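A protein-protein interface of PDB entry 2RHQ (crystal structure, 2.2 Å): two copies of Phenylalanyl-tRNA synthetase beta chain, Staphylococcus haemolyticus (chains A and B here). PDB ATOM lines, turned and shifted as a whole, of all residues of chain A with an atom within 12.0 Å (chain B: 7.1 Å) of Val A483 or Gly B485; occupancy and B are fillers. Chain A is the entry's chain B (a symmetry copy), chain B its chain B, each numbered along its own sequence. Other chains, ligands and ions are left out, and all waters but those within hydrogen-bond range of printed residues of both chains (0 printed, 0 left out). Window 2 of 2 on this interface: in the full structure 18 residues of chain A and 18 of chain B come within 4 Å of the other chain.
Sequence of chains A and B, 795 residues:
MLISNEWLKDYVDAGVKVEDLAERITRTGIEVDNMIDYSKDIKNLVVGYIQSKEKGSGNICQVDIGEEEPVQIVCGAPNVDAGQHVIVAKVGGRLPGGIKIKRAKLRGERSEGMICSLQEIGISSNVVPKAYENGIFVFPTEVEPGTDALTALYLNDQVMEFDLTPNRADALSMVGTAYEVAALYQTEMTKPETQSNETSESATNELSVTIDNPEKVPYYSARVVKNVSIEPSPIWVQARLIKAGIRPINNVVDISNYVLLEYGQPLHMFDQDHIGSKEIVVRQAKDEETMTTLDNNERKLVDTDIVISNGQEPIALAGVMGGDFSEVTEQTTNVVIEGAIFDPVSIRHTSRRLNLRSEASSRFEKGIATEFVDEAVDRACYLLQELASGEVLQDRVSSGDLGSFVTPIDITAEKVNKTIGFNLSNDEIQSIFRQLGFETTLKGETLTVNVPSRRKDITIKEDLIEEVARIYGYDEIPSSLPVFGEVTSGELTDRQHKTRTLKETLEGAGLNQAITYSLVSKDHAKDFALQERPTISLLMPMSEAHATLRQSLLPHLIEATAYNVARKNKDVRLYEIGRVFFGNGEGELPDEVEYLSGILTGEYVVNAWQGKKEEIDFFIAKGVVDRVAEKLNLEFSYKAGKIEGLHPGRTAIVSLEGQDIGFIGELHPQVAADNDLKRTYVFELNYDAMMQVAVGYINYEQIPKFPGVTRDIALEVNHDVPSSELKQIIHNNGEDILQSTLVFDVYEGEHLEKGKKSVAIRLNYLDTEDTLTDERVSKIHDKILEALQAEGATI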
ATOM      1  N   LYS A 418     -37.401 -14.851  -1.380  1.00  0.00           N
ATOM      2  CA  LYS A 418     -36.909 -14.053  -0.250  1.00  0.00           C
ATOM      3  C   LYS A 418     -35.955 -14.828   0.671  1.00  0.00           C
ATOM      4  O   LYS A 418     -35.087 -14.228   1.302  1.00  0.00           O
ATOM      5  CB  LYS A 418     -38.094 -13.484   0.574  1.00  0.00           C
ATOM      6  CG  LYS A 418     -38.466 -14.305   1.839  1.00  0.00           C
ATOM      7  CD  LYS A 418     -39.565 -13.656   2.717  1.00  0.00           C
ATOM      8  CE  LYS A 418     -38.990 -12.755   3.826  1.00  0.00           C
ATOM      9  NZ  LYS A 418     -39.805 -11.496   4.073  1.00  0.00           N
ATOM     10  N   SER A 479     -24.987 -13.291  -5.353  1.00  0.00           N
ATOM     11  CA  SER A 479     -24.090 -12.795  -4.306  1.00  0.00           C
ATOM     12  C   SER A 479     -24.599 -11.409  -3.872  1.00  0.00           C
ATOM     13  O   SER A 479     -24.563 -10.465  -4.647  1.00  0.00           O
ATOM     14  CB  SER A 479     -22.671 -12.688  -4.882  1.00  0.00           C
ATOM     15  OG  SER A 479     -21.678 -12.519  -3.876  1.00  0.00           O
ATOM     16  N   SER A 480     -25.085 -11.309  -2.633  1.00  0.00           N
ATOM     17  CA  SER A 480     -25.447 -10.039  -2.032  1.00  0.00           C
ATOM     18  C   SER A 480     -24.855  -9.924  -0.610  1.00  0.00           C
ATOM     19  O   SER A 480     -24.143 -10.800  -0.151  1.00  0.00           O
ATOM     20  CB  SER A 480     -26.967  -9.883  -2.048  1.00  0.00           C
ATOM     21  OG  SER A 480     -27.635 -10.584  -0.992  1.00  0.00           O
ATOM     22  N   LEU A 481     -25.092  -8.797   0.060  1.00  0.00           N
ATOM     23  CA  LEU A 481     -24.619  -8.573   1.432  1.00  0.00           C
ATOM     24  C   LEU A 481     -25.776  -7.963   2.136  1.00  0.00           C
ATOM     25  O   LEU A 481     -26.490  -7.160   1.557  1.00  0.00           O
ATOM     26  CB  LEU A 481     -23.428  -7.623   1.478  1.00  0.00           C
ATOM     27  CG  LEU A 481     -22.081  -8.236   1.109  1.00  0.00           C
ATOM     28  CD1 LEU A 481     -21.095  -7.199   0.587  1.00  0.00           C
ATOM     29  CD2 LEU A 481     -21.540  -8.962   2.304  1.00  0.00           C
ATOM     30  N   PRO A 482     -26.001  -8.355   3.381  1.00  0.00           N
ATOM     31  CA  PRO A 482     -27.173  -7.793   4.029  1.00  0.00           C
ATOM     32  C   PRO A 482     -26.966  -6.307   4.457  1.00  0.00           C
ATOM     33  O   PRO A 482     -25.915  -5.944   4.999  1.00  0.00           O
ATOM     34  CB  PRO A 482     -27.354  -8.685   5.268  1.00  0.00           C
ATOM     35  CG  PRO A 482     -26.033  -9.303   5.512  1.00  0.00           C
ATOM     36  CD  PRO A 482     -25.232  -9.250   4.258  1.00  0.00           C
ATOM     37  N   VAL A 483     -27.998  -5.497   4.246  1.00  0.00           N
ATOM     38  CA  VAL A 483     -28.012  -4.082   4.639  1.00  0.00           C
ATOM     39  C   VAL A 483     -28.742  -3.923   5.964  1.00  0.00           C
ATOM     40  O   VAL A 483     -29.955  -4.076   6.028  1.00  0.00           O
ATOM     41  CB  VAL A 483     -28.755  -3.250   3.590  1.00  0.00           C
ATOM     42  CG1 VAL A 483     -28.664  -1.777   3.930  1.00  0.00           C
ATOM     43  CG2 VAL A 483     -28.176  -3.509   2.245  1.00  0.00           C
ATOM     44  N   PHE A 484     -28.011  -3.648   7.033  1.00  0.00           N
ATOM     45  CA  PHE A 484     -28.661  -3.506   8.302  1.00  0.00           C
ATOM     46  C   PHE A 484     -29.259  -2.085   8.453  1.00  0.00           C
ATOM     47  O   PHE A 484     -28.649  -1.075   8.023  1.00  0.00           O
ATOM     48  CB  PHE A 484     -27.694  -3.809   9.400  1.00  0.00           C
ATOM     49  CG  PHE A 484     -27.044  -5.147   9.262  1.00  0.00           C
ATOM     50  CD1 PHE A 484     -27.764  -6.310   9.494  1.00  0.00           C
ATOM     51  CD2 PHE A 484     -25.734  -5.252   8.892  1.00  0.00           C
ATOM     52  CE1 PHE A 484     -27.175  -7.542   9.363  1.00  0.00           C
ATOM     53  CE2 PHE A 484     -25.142  -6.502   8.768  1.00  0.00           C
ATOM     54  CZ  PHE A 484     -25.888  -7.634   9.002  1.00  0.00           C
ATOM     55  N   GLY A 485     -30.470  -2.042   9.012  1.00  0.00           N
ATOM     56  CA  GLY A 485     -31.267  -0.826   9.076  1.00  0.00           C
ATOM     57  C   GLY A 485     -31.083  -0.150  10.425  1.00  0.00           C
ATOM     58  O   GLY A 485     -31.221   1.063  10.530  1.00  0.00           O
ATOM     59  N   GLU A 486     -30.766  -0.938  11.448  1.00  0.00           N
ATOM     60  CA  GLU A 486     -30.223  -0.424  12.686  1.00  0.00           C
ATOM     61  C   GLU A 486     -28.703  -0.437  12.625  1.00  0.00           C
ATOM     62  O   GLU A 486     -28.075  -1.508  12.608  1.00  0.00           O
ATOM     63  CB  GLU A 486     -30.731  -1.236  13.884  1.00  0.00           C
ATOM     64  CG  GLU A 486     -29.708  -1.429  14.999  1.00  0.00           C
ATOM     65  CD  GLU A 486     -30.344  -1.658  16.371  1.00  0.00           C
ATOM     66  OE1 GLU A 486     -31.444  -1.111  16.611  1.00  0.00           O
ATOM     67  OE2 GLU A 486     -29.734  -2.371  17.210  1.00  0.00           O
ATOM     68  N   VAL A 487     -28.129   0.772  12.592  1.00  0.00           N
ATOM     69  CA  VAL A 487     -26.693   0.970  12.355  1.00  0.00           C
ATOM     70  C   VAL A 487     -25.889   1.085  13.643  1.00  0.00           C
ATOM     71  O   VAL A 487     -26.202   1.872  14.534  1.00  0.00           O
ATOM     72  CB  VAL A 487     -26.444   2.181  11.506  1.00  0.00           C
ATOM     73  CG1 VAL A 487     -24.970   2.416  11.344  1.00  0.00           C
ATOM     74  CG2 VAL A 487     -27.155   2.051  10.151  1.00  0.00           C
ATOM     75  N   THR A 488     -24.855   0.271  13.734  1.00  0.00           N
ATOM     76  CA  THR A 488     -23.946   0.309  14.848  1.00  0.00           C
ATOM     77  C   THR A 488     -22.564   0.152  14.249  1.00  0.00           C
ATOM     78  O   THR A 488     -22.385  -0.560  13.265  1.00  0.00           O
ATOM     79  CB  THR A 488     -24.162  -0.821  15.911  1.00  0.00           C
ATOM     80  OG1 THR A 488     -23.930  -2.087  15.297  1.00  0.00           O
ATOM     81  CG2 THR A 488     -25.522  -0.755  16.536  1.00  0.00           C
ATOM     82  N   VAL B 483     -28.011   4.449   6.269  1.00  0.00           N
ATOM     83  CA  VAL B 483     -27.937   3.028   5.904  1.00  0.00           C
ATOM     84  C   VAL B 483     -27.409   2.889   4.484  1.00  0.00           C
ATOM     85  O   VAL B 483     -28.100   3.220   3.529  1.00  0.00           O
ATOM     86  CB  VAL B 483     -29.331   2.397   5.952  1.00  0.00           C
ATOM     87  CG1 VAL B 483     -29.240   0.907   5.698  1.00  0.00           C
ATOM     88  CG2 VAL B 483     -29.953   2.660   7.276  1.00  0.00           C
ATOM     89  N   PHE B 484     -26.177   2.429   4.334  1.00  0.00           N
ATOM     90  CA  PHE B 484     -25.639   2.298   3.014  1.00  0.00           C
ATOM     91  C   PHE B 484     -26.117   0.978   2.359  1.00  0.00           C
ATOM     92  O   PHE B 484     -26.215  -0.080   3.027  1.00  0.00           O
ATOM     93  CB  PHE B 484     -24.147   2.370   3.066  1.00  0.00           C
ATOM     94  CG  PHE B 484     -23.639   3.599   3.747  1.00  0.00           C
ATOM     95  CD1 PHE B 484     -23.737   4.839   3.132  1.00  0.00           C
ATOM     96  CD2 PHE B 484     -23.082   3.529   4.992  1.00  0.00           C
ATOM     97  CE1 PHE B 484     -23.279   5.972   3.753  1.00  0.00           C
ATOM     98  CE2 PHE B 484     -22.614   4.679   5.613  1.00  0.00           C
ATOM     99  CZ  PHE B 484     -22.731   5.892   4.975  1.00  0.00           C
ATOM    100  N   GLY B 485     -26.458   1.081   1.072  1.00  0.00           N
ATOM    101  CA  GLY B 485     -27.096  -0.001   0.336  1.00  0.00           C
ATOM    102  C   GLY B 485     -26.055  -0.792  -0.439  1.00  0.00           C
ATOM    103  O   GLY B 485     -26.246  -1.974  -0.699  1.00  0.00           O
ATOM    104  N   GLU B 486     -24.954  -0.136  -0.798  1.00  0.00           N
ATOM    105  CA  GLU B 486     -23.748  -0.815  -1.217  1.00  0.00           C
ATOM    106  C   GLU B 486     -22.837  -1.030  -0.018  1.00  0.00           C
ATOM    107  O   GLU B 486     -22.292  -0.070   0.549  1.00  0.00           O
ATOM    108  CB  GLU B 486     -23.029  -0.023  -2.316  1.00  0.00           C
ATOM    109  CG  GLU B 486     -21.506  -0.069  -2.238  1.00  0.00           C
ATOM    110  CD  GLU B 486     -20.824   0.156  -3.590  1.00  0.00           C
ATOM    111  OE1 GLU B 486     -21.416  -0.233  -4.621  1.00  0.00           O
ATOM    112  OE2 GLU B 486     -19.692   0.705  -3.612  1.00  0.00           O
ATOM    113  N   VAL B 487     -22.686  -2.307   0.356  1.00  0.00           N
ATOM    114  CA  VAL B 487     -21.996  -2.705   1.588  1.00  0.00           C
ATOM    115  C   VAL B 487     -20.526  -3.034   1.365  1.00  0.00           C
ATOM    116  O   VAL B 487     -20.162  -3.825   0.497  1.00  0.00           O
ATOM    117  CB  VAL B 487     -22.671  -3.876   2.238  1.00  0.00           C
ATOM    118  CG1 VAL B 487     -21.905  -4.321   3.449  1.00  0.00           C
ATOM    119  CG2 VAL B 487     -24.131  -3.542   2.575  1.00  0.00           C
ATOM    120  N   THR B 488     -19.681  -2.396   2.154  1.00  0.00           N
ATOM    121  CA  THR B 488     -18.266  -2.652   2.129  1.00  0.00           C
ATOM    122  C   THR B 488     -17.831  -2.666   3.579  1.00  0.00           C
ATOM    123  O   THR B 488     -18.360  -1.921   4.399  1.00  0.00           O
ATOM    124  CB  THR B 488     -17.418  -1.582   1.361  1.00  0.00           C
ATOM    125  OG1 THR B 488     -17.548  -0.326   2.024  1.00  0.00           O
ATOM    126  CG2 THR B 488     -17.807  -1.484  -0.082  1.00  0.00           C
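Among the printed residues, merely in contact across the chains: Leu A481 with Val B487, Pro A482 with Val B487, Val A483 with Val B483, Val A483 with Phe B484, Val A483 with Gly B485, Phe A484 with Val B483 and Gly A485 with Val B483.
Of chain B, only Val B483 (3.3 Å), Phe B484 (3.1 Å) and Gly B485 (3.8 Å) come within 4 Å of Val A483.
Val B483 touches just these residues of chain A: Val A483, Phe A484 and Gly A485.
Val B487 touches two residues of chain A.
Of the printed residues of chain B, Phe A484 touches Val B483 (3.1 Å).
Of the printed residues of chain B, Leu A481 touches Val B487.
Printed residues of chain B within 4 Å of Gly A485: Val B483.
The nearest residue of chain A that does not touch Gly B485 is Leu A481 (5.7 Å).
Hydrophobic or aromatic side chains of chain A within 4 Å of the printed part of chain B: Leu A481 and Val A483.
Among the printed residues, 7 pairs touch across the chains.
Among the printed residues, no Asp or Glu carboxylate lies within 4 Å of a Lys or Arg side-chain nitrogen of the other chain.
Val A483 touches its own counterpart, Val B483.
Val A483 touches Phe B484, and with the chains exchanged Phe A484 touches Val B483.
Val A483 touches Gly B485, and with the chains exchanged Gly A485 touches Val B483.
Positions printed for both chains: 483, 484, 485, 486, 487 and 488.
Of the 7 pairs that touch across the chains among the printed residues, 5 have their exchanged pair printed and touching as well.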
